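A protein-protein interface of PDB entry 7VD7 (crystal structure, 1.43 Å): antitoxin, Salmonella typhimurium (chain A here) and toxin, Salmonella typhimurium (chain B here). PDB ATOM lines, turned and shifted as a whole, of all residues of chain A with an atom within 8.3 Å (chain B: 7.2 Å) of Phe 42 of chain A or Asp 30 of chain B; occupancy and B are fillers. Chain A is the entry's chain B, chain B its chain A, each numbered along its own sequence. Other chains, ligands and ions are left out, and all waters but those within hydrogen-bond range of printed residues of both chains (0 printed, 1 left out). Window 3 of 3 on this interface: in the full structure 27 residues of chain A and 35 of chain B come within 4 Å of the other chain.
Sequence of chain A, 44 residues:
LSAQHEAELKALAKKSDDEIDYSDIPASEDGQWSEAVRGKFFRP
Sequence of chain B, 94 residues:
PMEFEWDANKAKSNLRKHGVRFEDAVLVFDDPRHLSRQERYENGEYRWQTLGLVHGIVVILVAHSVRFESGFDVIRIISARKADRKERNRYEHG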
ATOM      1  N   ARG A  38     -27.411 -24.736 -23.708  1.00  0.00           N
ATOM      2  CA  ARG A  38     -28.075 -23.534 -23.142  1.00  0.00           C
ATOM      3  C   ARG A  38     -28.404 -23.879 -21.692  1.00  0.00           C
ATOM      4  O   ARG A  38     -28.857 -24.974 -21.395  1.00  0.00           O
ATOM      5  CB  ARG A  38     -29.307 -23.108 -23.940  1.00  0.00           C
ATOM      6  CG  ARG A  38     -29.819 -21.751 -23.489  1.00  0.00           C
ATOM      7  CD  ARG A  38     -30.909 -21.202 -24.372  1.00  0.00           C
ATOM      8  NE  ARG A  38     -30.535 -21.067 -25.793  1.00  0.00           N
ATOM      9  CZ  ARG A  38     -30.023 -19.983 -26.365  1.00  0.00           C
ATOM     10  NH1 ARG A  38     -29.673 -18.922 -25.660  1.00  0.00           N
ATOM     11  NH2 ARG A  38     -29.828 -19.947 -27.672  1.00  0.00           N
ATOM     12  N   GLY A  39     -28.092 -22.952 -20.793  1.00  0.00           N
ATOM     13  CA  GLY A  39     -28.412 -23.108 -19.360  1.00  0.00           C
ATOM     14  C   GLY A  39     -27.427 -24.016 -18.659  1.00  0.00           C
ATOM     15  O   GLY A  39     -27.752 -24.494 -17.549  1.00  0.00           O
ATOM     16  N   LYS A  40     -26.248 -24.304 -19.257  1.00  0.00           N
ATOM     17  CA  LYS A  40     -25.279 -25.320 -18.804  1.00  0.00           C
ATOM     18  C   LYS A  40     -24.926 -25.117 -17.324  1.00  0.00           C
ATOM     19  O   LYS A  40     -24.888 -26.076 -16.515  1.00  0.00           O
ATOM     20  CB  LYS A  40     -24.051 -25.215 -19.716  1.00  0.00           C
ATOM     21  CG  LYS A  40     -22.870 -26.048 -19.253  1.00  0.00           C
ATOM     22  CD  LYS A  40     -23.142 -27.532 -19.314  1.00  0.00           C
ATOM     23  CE  LYS A  40     -22.166 -28.357 -18.515  1.00  0.00           C
ATOM     24  NZ  LYS A  40     -22.529 -28.363 -17.081  1.00  0.00           N
ATOM     25  N   PHE A  41     -24.722 -23.879 -16.895  1.00  0.00           N
ATOM     26  CA  PHE A  41     -24.145 -23.578 -15.557  1.00  0.00           C
ATOM     27  C   PHE A  41     -25.185 -22.793 -14.753  1.00  0.00           C
ATOM     28  O   PHE A  41     -24.846 -22.151 -13.746  1.00  0.00           O
ATOM     29  CB  PHE A  41     -22.887 -22.726 -15.722  1.00  0.00           C
ATOM     30  CG  PHE A  41     -21.794 -23.392 -16.523  1.00  0.00           C
ATOM     31  CD1 PHE A  41     -21.120 -24.477 -15.992  1.00  0.00           C
ATOM     32  CD2 PHE A  41     -21.525 -22.995 -17.820  1.00  0.00           C
ATOM     33  CE1 PHE A  41     -20.208 -25.174 -16.766  1.00  0.00           C
ATOM     34  CE2 PHE A  41     -20.575 -23.664 -18.573  1.00  0.00           C
ATOM     35  CZ  PHE A  41     -19.878 -24.711 -18.028  1.00  0.00           C
ATOM     36  N   PHE A  42     -26.451 -22.822 -15.152  1.00  0.00           N
ATOM     37  CA  PHE A  42     -27.526 -22.125 -14.408  1.00  0.00           C
ATOM     38  C   PHE A  42     -27.825 -22.851 -13.092  1.00  0.00           C
ATOM     39  O   PHE A  42     -28.000 -24.106 -13.126  1.00  0.00           O
ATOM     40  CB  PHE A  42     -28.827 -22.020 -15.202  1.00  0.00           C
ATOM     41  CG  PHE A  42     -29.885 -21.235 -14.459  1.00  0.00           C
ATOM     42  CD1 PHE A  42     -29.784 -19.860 -14.266  1.00  0.00           C
ATOM     43  CD2 PHE A  42     -31.010 -21.891 -13.990  1.00  0.00           C
ATOM     44  CE1 PHE A  42     -30.753 -19.155 -13.542  1.00  0.00           C
ATOM     45  CE2 PHE A  42     -31.989 -21.193 -13.278  1.00  0.00           C
ATOM     46  CZ  PHE A  42     -31.874 -19.818 -13.078  1.00  0.00           C
ATOM     47  N   ARG A  43     -27.802 -22.116 -11.974  1.00  0.00           N
ATOM     48  CA  ARG A  43     -28.187 -22.713 -10.671  1.00  0.00           C
ATOM     49  C   ARG A  43     -29.294 -21.817 -10.127  1.00  0.00           C
ATOM     50  O   ARG A  43     -29.146 -20.607 -10.028  1.00  0.00           O
ATOM     51  CB  ARG A  43     -26.979 -22.888  -9.750  1.00  0.00           C
ATOM     52  CG  ARG A  43     -25.913 -23.852 -10.259  1.00  0.00           C
ATOM     53  CD  ARG A  43     -26.322 -25.317 -10.201  1.00  0.00           C
ATOM     54  NE  ARG A  43     -26.681 -25.855 -11.501  1.00  0.00           N
ATOM     55  CZ  ARG A  43     -25.817 -26.002 -12.509  1.00  0.00           C
ATOM     56  NH1 ARG A  43     -24.548 -25.644 -12.361  1.00  0.00           N
ATOM     57  NH2 ARG A  43     -26.225 -26.471 -13.674  1.00  0.00           N
ATOM     58  N   PRO A  44     -30.481 -22.365  -9.848  1.00  0.00           N
ATOM     59  CA  PRO A  44     -31.550 -21.532  -9.291  1.00  0.00           C
ATOM     60  C   PRO A  44     -31.386 -21.107  -7.817  1.00  0.00           C
ATOM     61  O   PRO A  44     -30.354 -21.251  -7.133  1.00  0.00           O
ATOM     62  CB  PRO A  44     -32.763 -22.453  -9.479  1.00  0.00           C
ATOM     63  CG  PRO A  44     -32.181 -23.860  -9.406  1.00  0.00           C
ATOM     64  CD  PRO A  44     -30.888 -23.743 -10.183  1.00  0.00           C
ATOM     65  N   PHE B   4     -16.634 -18.681  -7.891  1.00  0.00           N
ATOM     66  CA  PHE B   4     -15.933 -18.001  -8.996  1.00  0.00           C
ATOM     67  C   PHE B   4     -14.578 -17.521  -8.522  1.00  0.00           C
ATOM     68  O   PHE B   4     -14.418 -17.040  -7.356  1.00  0.00           O
ATOM     69  CB  PHE B   4     -16.743 -16.824  -9.522  1.00  0.00           C
ATOM     70  CG  PHE B   4     -18.050 -17.275 -10.074  1.00  0.00           C
ATOM     71  CD1 PHE B   4     -18.139 -17.797 -11.355  1.00  0.00           C
ATOM     72  CD2 PHE B   4     -19.155 -17.334  -9.275  1.00  0.00           C
ATOM     73  CE1 PHE B   4     -19.351 -18.232 -11.839  1.00  0.00           C
ATOM     74  CE2 PHE B   4     -20.371 -17.785  -9.762  1.00  0.00           C
ATOM     75  CZ  PHE B   4     -20.472 -18.222 -11.053  1.00  0.00           C
ATOM     76  N   ALA B  25     -19.268 -10.164 -15.623  1.00  0.00           N
ATOM     77  CA  ALA B  25     -19.110 -11.360 -16.463  1.00  0.00           C
ATOM     78  C   ALA B  25     -19.643 -12.563 -15.716  1.00  0.00           C
ATOM     79  O   ALA B  25     -20.348 -13.398 -16.344  1.00  0.00           O
ATOM     80  CB  ALA B  25     -17.642 -11.576 -16.822  1.00  0.00           C
ATOM     81  N   VAL B  26     -19.443 -12.658 -14.424  1.00  0.00           N
ATOM     82  CA  VAL B  26     -20.006 -13.744 -13.599  1.00  0.00           C
ATOM     83  C   VAL B  26     -21.520 -13.821 -13.749  1.00  0.00           C
ATOM     84  O   VAL B  26     -22.094 -14.910 -13.598  1.00  0.00           O
ATOM     85  CB  VAL B  26     -19.605 -13.647 -12.128  1.00  0.00           C
ATOM     86  CG1 VAL B  26     -20.292 -14.682 -11.232  1.00  0.00           C
ATOM     87  CG2 VAL B  26     -18.102 -13.717 -11.942  1.00  0.00           C
ATOM     88  N   LEU B  27     -22.176 -12.704 -13.989  1.00  0.00           N
ATOM     89  CA  LEU B  27     -23.641 -12.705 -14.031  1.00  0.00           C
ATOM     90  C   LEU B  27     -24.183 -13.395 -15.271  1.00  0.00           C
ATOM     91  O   LEU B  27     -25.344 -13.783 -15.218  1.00  0.00           O
ATOM     92  CB  LEU B  27     -24.143 -11.273 -13.981  1.00  0.00           C
ATOM     93  CG  LEU B  27     -23.730 -10.524 -12.722  1.00  0.00           C
ATOM     94  CD1 LEU B  27     -24.252  -9.099 -12.803  1.00  0.00           C
ATOM     95  CD2 LEU B  27     -24.159 -11.229 -11.429  1.00  0.00           C
ATOM     96  N   VAL B  28     -23.380 -13.733 -16.272  1.00  0.00           N
ATOM     97  CA  VAL B  28     -23.921 -14.482 -17.425  1.00  0.00           C
ATOM     98  C   VAL B  28     -24.442 -15.835 -16.931  1.00  0.00           C
ATOM     99  O   VAL B  28     -25.392 -16.345 -17.527  1.00  0.00           O
ATOM    100  CB  VAL B  28     -22.898 -14.702 -18.554  1.00  0.00           C
ATOM    101  CG1 VAL B  28     -22.447 -13.366 -19.086  1.00  0.00           C
ATOM    102  CG2 VAL B  28     -21.764 -15.675 -18.260  1.00  0.00           C
ATOM    103  N   PHE B  29     -23.896 -16.409 -15.865  1.00  0.00           N
ATOM    104  CA  PHE B  29     -24.296 -17.760 -15.419  1.00  0.00           C
ATOM    105  C   PHE B  29     -25.656 -17.713 -14.700  1.00  0.00           C
ATOM    106  O   PHE B  29     -26.303 -18.757 -14.567  1.00  0.00           O
ATOM    107  CB  PHE B  29     -23.189 -18.393 -14.579  1.00  0.00           C
ATOM    108  CG  PHE B  29     -21.895 -18.468 -15.341  1.00  0.00           C
ATOM    109  CD1 PHE B  29     -21.771 -19.253 -16.470  1.00  0.00           C
ATOM    110  CD2 PHE B  29     -20.876 -17.614 -15.038  1.00  0.00           C
ATOM    111  CE1 PHE B  29     -20.603 -19.242 -17.203  1.00  0.00           C
ATOM    112  CE2 PHE B  29     -19.701 -17.615 -15.754  1.00  0.00           C
ATOM    113  CZ  PHE B  29     -19.547 -18.453 -16.826  1.00  0.00           C
ATOM    114  N   ASP B  30     -26.075 -16.512 -14.286  1.00  0.00           N
ATOM    115  CA  ASP B  30     -27.409 -16.268 -13.667  1.00  0.00           C
ATOM    116  C   ASP B  30     -28.456 -16.029 -14.753  1.00  0.00           C
ATOM    117  O   ASP B  30     -29.651 -15.902 -14.406  1.00  0.00           O
ATOM    118  CB  ASP B  30     -27.351 -15.136 -12.633  1.00  0.00           C
ATOM    119  CG  ASP B  30     -26.335 -15.314 -11.507  1.00  0.00           C
ATOM    120  OD1 ASP B  30     -26.071 -16.477 -11.170  1.00  0.00           O
ATOM    121  OD2 ASP B  30     -25.905 -14.278 -10.911  1.00  0.00           O
ATOM    122  N   ASP B  31     -28.086 -15.855 -16.012  1.00  0.00           N
ATOM    123  CA  ASP B  31     -29.067 -15.744 -17.115  1.00  0.00           C
ATOM    124  C   ASP B  31     -29.484 -17.164 -17.501  1.00  0.00           C
ATOM    125  O   ASP B  31     -28.648 -17.959 -17.967  1.00  0.00           O
ATOM    126  CB  ASP B  31     -28.399 -15.050 -18.288  1.00  0.00           C
ATOM    127  CG  ASP B  31     -29.244 -14.978 -19.526  1.00  0.00           C
ATOM    128  OD1 ASP B  31     -30.388 -15.481 -19.502  1.00  0.00           O
ATOM    129  OD2 ASP B  31     -28.747 -14.504 -20.544  1.00  0.00           O
ATOM    130  N   PRO B  32     -30.718 -17.616 -17.295  1.00  0.00           N
ATOM    131  CA  PRO B  32     -31.098 -19.002 -17.570  1.00  0.00           C
ATOM    132  C   PRO B  32     -30.912 -19.354 -19.052  1.00  0.00           C
ATOM    133  O   PRO B  32     -30.832 -20.536 -19.379  1.00  0.00           O
ATOM    134  CB  PRO B  32     -32.588 -19.083 -17.172  1.00  0.00           C
ATOM    135  CG  PRO B  32     -33.068 -17.693 -17.151  1.00  0.00           C
ATOM    136  CD  PRO B  32     -31.870 -16.825 -16.845  1.00  0.00           C
ATOM    137  N   ARG B  33     -30.801 -18.364 -19.931  1.00  0.00           N
ATOM    138  CA  ARG B  33     -30.675 -18.586 -21.386  1.00  0.00           C
ATOM    139  C   ARG B  33     -29.203 -18.533 -21.807  1.00  0.00           C
ATOM    140  O   ARG B  33     -28.927 -18.580 -22.999  1.00  0.00           O
ATOM    141  CB  ARG B  33     -31.557 -17.572 -22.122  1.00  0.00           C
ATOM    142  CG  ARG B  33     -33.027 -18.006 -22.043  1.00  0.00           C
ATOM    143  CD  ARG B  33     -33.966 -17.339 -22.971  1.00  0.00           C
ATOM    144  NE  ARG B  33     -33.488 -17.476 -24.341  1.00  0.00           N
ATOM    145  CZ  ARG B  33     -33.702 -18.509 -25.165  1.00  0.00           C
ATOM    146  NH1 ARG B  33     -34.349 -19.598 -24.785  1.00  0.00           N
ATOM    147  NH2 ARG B  33     -33.210 -18.433 -26.388  1.00  0.00           N
ATOM    148  N   HIS B  34     -28.266 -18.423 -20.885  1.00  0.00           N
ATOM    149  CA  HIS B  34     -26.860 -18.395 -21.321  1.00  0.00           C
ATOM    150  C   HIS B  34     -26.513 -19.592 -22.212  1.00  0.00           C
ATOM    151  O   HIS B  34     -27.035 -20.672 -21.999  1.00  0.00           O
ATOM    152  CB  HIS B  34     -25.908 -18.199 -20.156  1.00  0.00           C
ATOM    153  CG  HIS B  34     -25.745 -19.365 -19.263  1.00  0.00           C
ATOM    154  ND1 HIS B  34     -26.309 -19.397 -18.018  1.00  0.00           N
ATOM    155  CD2 HIS B  34     -25.051 -20.535 -19.351  1.00  0.00           C
ATOM    156  CE1 HIS B  34     -26.005 -20.522 -17.391  1.00  0.00           C
ATOM    157  NE2 HIS B  34     -25.238 -21.261 -18.183  1.00  0.00           N
ATOM    158  N   LEU B  53     -26.815 -12.417 -21.099  1.00  0.00           N
ATOM    159  CA  LEU B  53     -27.285 -11.038 -20.958  1.00  0.00           C
ATOM    160  C   LEU B  53     -26.988 -10.560 -19.542  1.00  0.00           C
ATOM    161  O   LEU B  53     -27.363 -11.278 -18.566  1.00  0.00           O
ATOM    162  CB  LEU B  53     -28.786 -11.004 -21.247  1.00  0.00           C
ATOM    163  CG  LEU B  53     -29.460  -9.640 -21.169  1.00  0.00           C
ATOM    164  CD1 LEU B  53     -28.965  -8.738 -22.287  1.00  0.00           C
ATOM    165  CD2 LEU B  53     -30.996  -9.799 -21.237  1.00  0.00           C
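Arg 38 of chain A touches His 34 of chain B (CA to O, 3.3 Å).
Gly 39 of chain A touches Pro 32 of chain B.
Phe 29 of chain B touches Phe 41 of chain A (CD1 to CB, 3.7 Å).
Phe 29 of chain B touches Phe 42 of chain A.
Asp 30 of chain B touches Phe 42 of chain A.
Phe 42 of chain A touches Pro 32 of chain B.
N of Phe 42 of chain A touches CE1 of His 34 of chain B, 3.2 Å away.
The backbone NH of Arg 33 of chain B lies within hydrogen-bond range of the side-chain carboxylate of Asp 31 of chain B.
O of Lys 40 of chain A is in hydrogen-bond range of NH2 of Arg 43 of chain A.
ND1 of His 34 of chain B is in hydrogen-bond range of O of Asp 31 of chain B, at 2.7 Å.
O of Val 28 of chain B sits at hydrogen-bond distance from ND1 of His 34 of chain B (3.2 Å).
Phe 42 of chain A touches four residues of chain B.
Printed residues of chain A within 4 Å of Asp 30 of chain B: Phe 42.
Printed residues of chain B within 4 Å of Lys 40 of chain A: His 34 (3.4 Å).
Of the printed residues of chain B, Phe 41 of chain A touches Phe 29 (3.7 Å) and His 34 (3.0 Å).
Of the printed residues of chain B, Arg 38 of chain A touches Arg 33 (2.8 Å) and His 34 (3.3 Å).
Ala 25 of chain B touches none of the printed residues of chain A.
The nearest printed residue of chain A that does not touch Phe 29 of chain B is Arg 43 of chain A (4.5 Å).
N of Phe 41 of chain A lies within hydrogen-bond range of NE2 of His 34 of chain B, 3.0 Å away.
O of His 34 of chain B is in hydrogen-bond range of N of Gly 39 of chain A, at 2.8 Å.
A ring nitrogen (NE2) of His 34 of chain B is in hydrogen-bond range of the backbone NH (N) of Lys 40 of chain A (3.4 Å).
O of Arg 33 of chain B is in hydrogen-bond range of NH1 of Arg 38 of chain A (2.8 Å).
Hydrophobic or aromatic side chains of chain A that line the printed part of chain B: Phe 41 and Phe 42.
Along chain A the printed residues that touch a printed residue of chain B span positions 38 to 42.
Hydrophobic or aromatic side chains of chain B that line the printed part of chain A: Phe 29 and His 34.
Along chain B the printed residues that touch a printed residue of chain A span positions 29 to 34.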
